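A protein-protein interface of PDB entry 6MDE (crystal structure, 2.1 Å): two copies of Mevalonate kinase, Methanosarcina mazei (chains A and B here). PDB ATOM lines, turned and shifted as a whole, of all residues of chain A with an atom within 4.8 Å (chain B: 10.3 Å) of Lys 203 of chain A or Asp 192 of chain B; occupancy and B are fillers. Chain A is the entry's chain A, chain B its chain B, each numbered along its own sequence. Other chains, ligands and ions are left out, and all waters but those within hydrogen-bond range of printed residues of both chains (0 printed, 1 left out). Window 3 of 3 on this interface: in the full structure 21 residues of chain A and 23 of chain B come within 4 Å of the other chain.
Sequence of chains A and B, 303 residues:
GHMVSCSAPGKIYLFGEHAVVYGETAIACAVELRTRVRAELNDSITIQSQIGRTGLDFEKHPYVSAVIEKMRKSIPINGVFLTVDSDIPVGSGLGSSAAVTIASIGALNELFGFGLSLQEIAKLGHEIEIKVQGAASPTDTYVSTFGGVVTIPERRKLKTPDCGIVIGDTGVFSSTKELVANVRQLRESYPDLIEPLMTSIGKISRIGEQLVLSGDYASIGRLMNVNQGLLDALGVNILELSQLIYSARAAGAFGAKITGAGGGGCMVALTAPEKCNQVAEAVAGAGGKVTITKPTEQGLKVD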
ATOM      1  N   GLU A  24      17.808  35.514  22.496  1.00  0.00           N
ATOM      2  CA  GLU A  24      17.087  35.350  21.241  1.00  0.00           C
ATOM      3  C   GLU A  24      16.403  36.652  20.844  1.00  0.00           C
ATOM      4  O   GLU A  24      16.203  37.550  21.656  1.00  0.00           O
ATOM      5  CB  GLU A  24      16.059  34.215  21.341  1.00  0.00           C
ATOM      6  CG  GLU A  24      16.686  32.830  21.560  1.00  0.00           C
ATOM      7  CD  GLU A  24      17.603  32.375  20.412  1.00  0.00           C
ATOM      8  OE1 GLU A  24      17.440  32.856  19.274  1.00  0.00           O
ATOM      9  OE2 GLU A  24      18.493  31.531  20.651  1.00  0.00           O
ATOM     10  N   THR A 199      15.751  28.579  20.990  1.00  0.00           N
ATOM     11  CA  THR A 199      16.301  28.874  19.670  1.00  0.00           C
ATOM     12  C   THR A 199      15.196  28.939  18.620  1.00  0.00           C
ATOM     13  O   THR A 199      15.205  29.816  17.753  1.00  0.00           O
ATOM     14  CB  THR A 199      17.344  27.817  19.284  1.00  0.00           C
ATOM     15  OG1 THR A 199      18.339  27.720  20.307  1.00  0.00           O
ATOM     16  CG2 THR A 199      18.011  28.181  17.978  1.00  0.00           C
ATOM     17  N   SER A 200      14.242  28.008  18.681  1.00  0.00           N
ATOM     18  CA  SER A 200      13.100  28.027  17.777  1.00  0.00           C
ATOM     19  C   SER A 200      12.299  29.317  17.892  1.00  0.00           C
ATOM     20  O   SER A 200      11.892  29.893  16.877  1.00  0.00           O
ATOM     21  CB  SER A 200      12.198  26.835  18.076  1.00  0.00           C
ATOM     22  OG  SER A 200      12.898  25.650  17.790  1.00  0.00           O
ATOM     23  N   ILE A 201      12.011  29.758  19.113  1.00  0.00           N
ATOM     24  CA  ILE A 201      11.283  31.010  19.248  1.00  0.00           C
ATOM     25  C   ILE A 201      12.072  32.134  18.584  1.00  0.00           C
ATOM     26  O   ILE A 201      11.510  32.942  17.833  1.00  0.00           O
ATOM     27  CB  ILE A 201      10.974  31.305  20.730  1.00  0.00           C
ATOM     28  CG1 ILE A 201       9.876  30.367  21.244  1.00  0.00           C
ATOM     29  CG2 ILE A 201      10.562  32.772  20.913  1.00  0.00           C
ATOM     30  CD1 ILE A 201       9.672  30.450  22.792  1.00  0.00           C
ATOM     31  N   GLY A 202      13.393  32.159  18.798  1.00  0.00           N
ATOM     32  CA  GLY A 202      14.235  33.137  18.124  1.00  0.00           C
ATOM     33  C   GLY A 202      14.127  33.054  16.613  1.00  0.00           C
ATOM     34  O   GLY A 202      13.944  34.072  15.933  1.00  0.00           O
ATOM     35  N   LYS A 203      14.202  31.832  16.070  1.00  0.00           N
ATOM     36  CA  LYS A 203      14.033  31.637  14.633  1.00  0.00           C
ATOM     37  C   LYS A 203      12.696  32.185  14.154  1.00  0.00           C
ATOM     38  O   LYS A 203      12.603  32.745  13.053  1.00  0.00           O
ATOM     39  CB  LYS A 203      14.146  30.154  14.281  1.00  0.00           C
ATOM     40  CG  LYS A 203      15.445  29.738  13.637  1.00  0.00           C
ATOM     41  CD  LYS A 203      15.693  28.262  13.867  1.00  0.00           C
ATOM     42  CE  LYS A 203      17.152  27.898  13.666  1.00  0.00           C
ATOM     43  NZ  LYS A 203      17.455  26.540  14.189  1.00  0.00           N
ATOM     44  N   ILE A 204      11.641  32.036  14.962  1.00  0.00           N
ATOM     45  CA  ILE A 204      10.348  32.563  14.542  1.00  0.00           C
ATOM     46  C   ILE A 204      10.439  34.067  14.340  1.00  0.00           C
ATOM     47  O   ILE A 204       9.957  34.596  13.336  1.00  0.00           O
ATOM     48  CB  ILE A 204       9.246  32.198  15.549  1.00  0.00           C
ATOM     49  CG1 ILE A 204       9.031  30.691  15.554  1.00  0.00           C
ATOM     50  CG2 ILE A 204       7.943  32.915  15.192  1.00  0.00           C
ATOM     51  CD1 ILE A 204       7.932  30.251  16.458  1.00  0.00           C
ATOM     52  N   SER A 205      11.082  34.774  15.273  1.00  0.00           N
ATOM     53  CA  SER A 205      11.165  36.225  15.161  1.00  0.00           C
ATOM     54  C   SER A 205      11.929  36.637  13.909  1.00  0.00           C
ATOM     55  O   SER A 205      11.577  37.628  13.259  1.00  0.00           O
ATOM     56  CB  SER A 205      11.844  36.828  16.394  1.00  0.00           C
ATOM     57  OG  SER A 205      11.081  36.600  17.570  1.00  0.00           O
ATOM     58  N   ARG A 206      12.976  35.884  13.555  1.00  0.00           N
ATOM     59  CA  ARG A 206      13.806  36.278  12.424  1.00  0.00           C
ATOM     60  C   ARG A 206      13.112  35.994  11.100  1.00  0.00           C
ATOM     61  O   ARG A 206      13.232  36.785  10.157  1.00  0.00           O
ATOM     62  CB  ARG A 206      15.164  35.588  12.520  1.00  0.00           C
ATOM     63  CG  ARG A 206      15.971  36.110  13.727  1.00  0.00           C
ATOM     64  CD  ARG A 206      17.424  35.662  13.709  1.00  0.00           C
ATOM     65  NE  ARG A 206      17.568  34.233  13.975  1.00  0.00           N
ATOM     66  CZ  ARG A 206      17.536  33.691  15.190  1.00  0.00           C
ATOM     67  NH1 ARG A 206      17.668  32.377  15.329  1.00  0.00           N
ATOM     68  NH2 ARG A 206      17.376  34.464  16.267  1.00  0.00           N
ATOM     69  N   ILE A 207      12.338  34.909  11.028  1.00  0.00           N
ATOM     70  CA  ILE A 207      11.418  34.736   9.903  1.00  0.00           C
ATOM     71  C   ILE A 207      10.375  35.846   9.905  1.00  0.00           C
ATOM     72  O   ILE A 207      10.058  36.420   8.861  1.00  0.00           O
ATOM     73  CB  ILE A 207      10.743  33.347   9.945  1.00  0.00           C
ATOM     74  CG1 ILE A 207      11.771  32.219   9.962  1.00  0.00           C
ATOM     75  CG2 ILE A 207       9.779  33.182   8.744  1.00  0.00           C
ATOM     76  CD1 ILE A 207      11.155  30.835  10.018  1.00  0.00           C
ATOM     77  N   GLN B 185       3.083  19.836   5.436  1.00  0.00           N
ATOM     78  CA  GLN B 185       3.157  21.088   4.689  1.00  0.00           C
ATOM     79  C   GLN B 185       3.863  22.168   5.502  1.00  0.00           C
ATOM     80  O   GLN B 185       4.747  22.871   4.993  1.00  0.00           O
ATOM     81  CB  GLN B 185       1.753  21.542   4.280  1.00  0.00           C
ATOM     82  CG  GLN B 185       1.623  23.020   3.880  1.00  0.00           C
ATOM     83  CD  GLN B 185       2.390  23.401   2.610  1.00  0.00           C
ATOM     84  OE1 GLN B 185       3.483  23.967   2.678  1.00  0.00           O
ATOM     85  NE2 GLN B 185       1.811  23.104   1.450  1.00  0.00           N
ATOM     86  N   LEU B 186       3.486  22.311   6.773  1.00  0.00           N
ATOM     87  CA  LEU B 186       4.128  23.288   7.645  1.00  0.00           C
ATOM     88  C   LEU B 186       5.628  23.039   7.738  1.00  0.00           C
ATOM     89  O   LEU B 186       6.426  23.982   7.695  1.00  0.00           O
ATOM     90  CB  LEU B 186       3.482  23.229   9.030  1.00  0.00           C
ATOM     91  CG  LEU B 186       3.945  24.225  10.091  1.00  0.00           C
ATOM     92  CD1 LEU B 186       3.624  25.641   9.643  1.00  0.00           C
ATOM     93  CD2 LEU B 186       3.222  23.899  11.407  1.00  0.00           C
ATOM     94  N   ARG B 187       6.024  21.768   7.850  1.00  0.00           N
ATOM     95  CA  ARG B 187       7.441  21.419   7.900  1.00  0.00           C
ATOM     96  C   ARG B 187       8.158  21.834   6.622  1.00  0.00           C
ATOM     97  O   ARG B 187       9.299  22.310   6.668  1.00  0.00           O
ATOM     98  CB  ARG B 187       7.584  19.917   8.137  1.00  0.00           C
ATOM     99  CG  ARG B 187       9.006  19.401   8.191  1.00  0.00           C
ATOM    100  CD  ARG B 187       8.997  17.923   8.592  1.00  0.00           C
ATOM    101  NE  ARG B 187      10.336  17.384   8.819  1.00  0.00           N
ATOM    102  CZ  ARG B 187      11.143  16.958   7.852  1.00  0.00           C
ATOM    103  NH1 ARG B 187      10.749  17.010   6.584  1.00  0.00           N
ATOM    104  NH2 ARG B 187      12.346  16.480   8.153  1.00  0.00           N
ATOM    105  N   GLU B 188       7.502  21.660   5.471  1.00  0.00           N
ATOM    106  CA  GLU B 188       8.092  22.065   4.199  1.00  0.00           C
ATOM    107  C   GLU B 188       8.135  23.580   4.055  1.00  0.00           C
ATOM    108  O   GLU B 188       9.077  24.119   3.458  1.00  0.00           O
ATOM    109  CB  GLU B 188       7.309  21.454   3.037  1.00  0.00           C
ATOM    110  CG  GLU B 188       7.752  20.052   2.654  1.00  0.00           C
ATOM    111  CD  GLU B 188       6.611  19.216   2.089  1.00  0.00           C
ATOM    112  OE1 GLU B 188       5.581  19.798   1.674  1.00  0.00           O
ATOM    113  OE2 GLU B 188       6.741  17.974   2.059  1.00  0.00           O
ATOM    114  N   SER B 189       7.134  24.285   4.590  1.00  0.00           N
ATOM    115  CA  SER B 189       7.153  25.744   4.520  1.00  0.00           C
ATOM    116  C   SER B 189       8.317  26.332   5.313  1.00  0.00           C
ATOM    117  O   SER B 189       8.990  27.262   4.850  1.00  0.00           O
ATOM    118  CB  SER B 189       5.828  26.311   5.019  1.00  0.00           C
ATOM    119  OG  SER B 189       4.835  26.234   4.021  1.00  0.00           O
ATOM    120  N   TYR B 190       8.582  25.807   6.506  1.00  0.00           N
ATOM    121  CA  TYR B 190       9.597  26.372   7.392  1.00  0.00           C
ATOM    122  C   TYR B 190      10.497  25.265   7.922  1.00  0.00           C
ATOM    123  O   TYR B 190      10.525  24.989   9.127  1.00  0.00           O
ATOM    124  CB  TYR B 190       8.932  27.144   8.531  1.00  0.00           C
ATOM    125  CG  TYR B 190       7.956  28.222   8.093  1.00  0.00           C
ATOM    126  CD1 TYR B 190       8.410  29.435   7.560  1.00  0.00           C
ATOM    127  CD2 TYR B 190       6.586  28.049   8.239  1.00  0.00           C
ATOM    128  CE1 TYR B 190       7.518  30.437   7.173  1.00  0.00           C
ATOM    129  CE2 TYR B 190       5.688  29.041   7.859  1.00  0.00           C
ATOM    130  CZ  TYR B 190       6.158  30.229   7.328  1.00  0.00           C
ATOM    131  OH  TYR B 190       5.258  31.200   6.953  1.00  0.00           O
ATOM    132  N   PRO B 191      11.265  24.618   7.045  1.00  0.00           N
ATOM    133  CA  PRO B 191      12.039  23.446   7.490  1.00  0.00           C
ATOM    134  C   PRO B 191      13.051  23.762   8.569  1.00  0.00           C
ATOM    135  O   PRO B 191      13.227  22.975   9.505  1.00  0.00           O
ATOM    136  CB  PRO B 191      12.714  22.975   6.196  1.00  0.00           C
ATOM    137  CG  PRO B 191      12.732  24.192   5.327  1.00  0.00           C
ATOM    138  CD  PRO B 191      11.458  24.896   5.613  1.00  0.00           C
ATOM    139  N   ASP B 192      13.727  24.901   8.452  1.00  0.00           N
ATOM    140  CA  ASP B 192      14.712  25.307   9.442  1.00  0.00           C
ATOM    141  C   ASP B 192      14.074  25.525  10.810  1.00  0.00           C
ATOM    142  O   ASP B 192      14.750  25.381  11.830  1.00  0.00           O
ATOM    143  CB  ASP B 192      15.422  26.576   8.935  1.00  0.00           C
ATOM    144  CG  ASP B 192      16.610  26.977   9.790  1.00  0.00           C
ATOM    145  OD1 ASP B 192      17.473  26.114  10.081  1.00  0.00           O
ATOM    146  OD2 ASP B 192      16.680  28.169  10.167  1.00  0.00           O
ATOM    147  N   LEU B 193      12.778  25.836  10.850  1.00  0.00           N
ATOM    148  CA  LEU B 193      12.061  26.055  12.097  1.00  0.00           C
ATOM    149  C   LEU B 193      11.375  24.785  12.609  1.00  0.00           C
ATOM    150  O   LEU B 193      11.483  24.455  13.794  1.00  0.00           O
ATOM    151  CB  LEU B 193      11.038  27.176  11.901  1.00  0.00           C
ATOM    152  CG  LEU B 193      10.000  27.342  13.015  1.00  0.00           C
ATOM    153  CD1 LEU B 193      10.684  27.668  14.351  1.00  0.00           C
ATOM    154  CD2 LEU B 193       9.026  28.440  12.656  1.00  0.00           C
ATOM    155  N   ILE B 194      10.682  24.051  11.734  1.00  0.00           N
ATOM    156  CA  ILE B 194       9.823  22.958  12.185  1.00  0.00           C
ATOM    157  C   ILE B 194      10.620  21.685  12.441  1.00  0.00           C
ATOM    158  O   ILE B 194      10.284  20.902  13.341  1.00  0.00           O
ATOM    159  CB  ILE B 194       8.690  22.718  11.171  1.00  0.00           C
ATOM    160  CG1 ILE B 194       7.876  24.000  10.997  1.00  0.00           C
ATOM    161  CG2 ILE B 194       7.796  21.543  11.609  1.00  0.00           C
ATOM    162  CD1 ILE B 194       7.299  24.519  12.291  1.00  0.00           C
ATOM    163  N   GLU B 195      11.657  21.429  11.642  1.00  0.00           N
ATOM    164  CA  GLU B 195      12.430  20.208  11.846  1.00  0.00           C
ATOM    165  C   GLU B 195      13.095  20.165  13.218  1.00  0.00           C
ATOM    166  O   GLU B 195      13.079  19.087  13.840  1.00  0.00           O
ATOM    167  CB  GLU B 195      13.452  20.035  10.712  1.00  0.00           C
ATOM    168  CG  GLU B 195      12.787  19.763   9.357  1.00  0.00           C
ATOM    169  CD  GLU B 195      13.781  19.466   8.234  1.00  0.00           C
ATOM    170  OE1 GLU B 195      15.010  19.484   8.485  1.00  0.00           O
ATOM    171  OE2 GLU B 195      13.325  19.206   7.096  1.00  0.00           O
ATOM    172  N   PRO B 196      13.676  21.252  13.743  1.00  0.00           N
ATOM    173  CA  PRO B 196      14.128  21.233  15.154  1.00  0.00           C
ATOM    174  C   PRO B 196      13.018  20.974  16.169  1.00  0.00           C
ATOM    175  O   PRO B 196      13.306  20.481  17.270  1.00  0.00           O
ATOM    176  CB  PRO B 196      14.729  22.634  15.341  1.00  0.00           C
ATOM    177  CG  PRO B 196      15.181  23.025  13.957  1.00  0.00           C
ATOM    178  CD  PRO B 196      14.149  22.454  13.034  1.00  0.00           C
ATOM    179  N   LEU B 197      11.768  21.336  15.859  1.00  0.00           N
ATOM    180  CA  LEU B 197      10.668  21.001  16.761  1.00  0.00           C
ATOM    181  C   LEU B 197      10.447  19.500  16.803  1.00  0.00           C
ATOM    182  O   LEU B 197      10.173  18.946  17.869  1.00  0.00           O
ATOM    183  CB  LEU B 197       9.379  21.710  16.348  1.00  0.00           C
ATOM    184  CG  LEU B 197       9.341  23.232  16.396  1.00  0.00           C
ATOM    185  CD1 LEU B 197       7.894  23.675  16.303  1.00  0.00           C
ATOM    186  CD2 LEU B 197      10.002  23.759  17.668  1.00  0.00           C
ATOM    187  N   MET B 198      10.560  18.828  15.649  1.00  0.00           N
ATOM    188  CA  MET B 198      10.492  17.367  15.627  1.00  0.00           C
ATOM    189  C   MET B 198      11.636  16.740  16.409  1.00  0.00           C
ATOM    190  O   MET B 198      11.471  15.671  17.010  1.00  0.00           O
ATOM    191  CB  MET B 198      10.525  16.856  14.192  1.00  0.00           C
ATOM    192  CG  MET B 198       9.453  17.423  13.322  1.00  0.00           C
ATOM    193  SD  MET B 198       7.823  16.836  13.808  1.00  0.00           S
ATOM    194  CE  MET B 198       6.866  17.798  12.636  1.00  0.00           C
ATOM    195  N   THR B 199      12.823  17.346  16.345  1.00  0.00           N
ATOM    196  CA  THR B 199      13.951  16.883  17.150  1.00  0.00           C
ATOM    197  C   THR B 199      13.640  16.991  18.640  1.00  0.00           C
ATOM    198  O   THR B 199      13.900  16.060  19.413  1.00  0.00           O
ATOM    199  CB  THR B 199      15.194  17.706  16.806  1.00  0.00           C
ATOM    200  OG1 THR B 199      15.356  17.756  15.386  1.00  0.00           O
ATOM    201  CG2 THR B 199      16.434  17.090  17.434  1.00  0.00           C
ATOM    202  N   SER B 200      13.082  18.130  19.053  1.00  0.00           N
ATOM    203  CA  SER B 200      12.675  18.316  20.437  1.00  0.00           C
ATOM    204  C   SER B 200      11.678  17.249  20.880  1.00  0.00           C
ATOM    205  O   SER B 200      11.780  16.727  21.992  1.00  0.00           O
ATOM    206  CB  SER B 200      12.084  19.710  20.608  1.00  0.00           C
ATOM    207  OG  SER B 200      12.917  20.660  19.998  1.00  0.00           O
ATOM    208  N   LYS B 203      13.622  14.262  21.632  1.00  0.00           N
ATOM    209  CA  LYS B 203      14.400  14.408  22.859  1.00  0.00           C
ATOM    210  C   LYS B 203      13.534  14.176  24.088  1.00  0.00           C
ATOM    211  O   LYS B 203      13.999  13.616  25.087  1.00  0.00           O
ATOM    212  CB  LYS B 203      15.039  15.792  22.919  1.00  0.00           C
ATOM    213  CG  LYS B 203      16.505  15.825  22.519  1.00  0.00           C
ATOM    214  CD  LYS B 203      17.048  17.238  22.619  1.00  0.00           C
ATOM    215  CE  LYS B 203      17.676  17.689  21.304  1.00  0.00           C
ATOM    216  NZ  LYS B 203      17.796  19.175  21.247  1.00  0.00           N
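Of the 10 printed residues of chain A, 4 touch a printed residue of chain B.
Along chain A the printed residues that touch a printed residue of chain B span positions 200 to 207.
Of the 17 printed residues of chain B, 4 touch a printed residue of chain A.
Hydrophobic or aromatic side chains of chain B that line the printed part of chain A: Tyr 190, Leu 193 and Leu 197.
Among the printed residues, no Asp or Glu carboxylate lies within 4 Å of a Lys or Arg side-chain nitrogen of the other chain.
Thr 199 of chain A touches none of the printed residues of chain B.
Of the printed residues of chain B, Ser 200 of chain A touches Leu 193 (3.6 Å) and Leu 197 (3.5 Å).
Ile 201 of chain A touches none of the printed residues of chain B.
Gly 202 of chain A touches none of the printed residues of chain B.
Of chain B, only Leu 193 (3.6 Å) comes within 4 Å of Ile 204 of chain A.
No residue of chain B comes within 4 Å of Ser 205 of chain A.
No residue of chain B comes within 4 Å of Arg 206 of chain A.
Of the printed residues of chain B, Ile 207 of chain A touches Tyr 190.
Printed residues of chain A within 4 Å of Tyr 190 of chain B: Ile 207 (3.9 Å).
Asp 192 of chain B touches just one residue of chain A: Lys 203 (3.5 Å).
Of the printed residues of chain A, Leu 193 of chain B touches Ser 200 and Ile 204.
Of the printed residues of chain A, Leu 197 of chain B touches Ser 200 (3.5 Å).
3 positions are printed for both chains.
CD1 of Leu 193 of chain B touches O of Ser 200 of chain A (3.6 Å).
Leu 197 of chain B touches Ser 200 of chain A (CD2 to OG, 3.5 Å).
CE of Lys 203 of chain A touches OD2 of Asp 192 of chain B, at 3.5 Å.
Ile 204 of chain A touches Leu 193 of chain B (CG1 to CD1, 3.6 Å).
Ile 207 of chain A touches Tyr 190 of chain B (CG2 to CE1, 3.9 Å).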
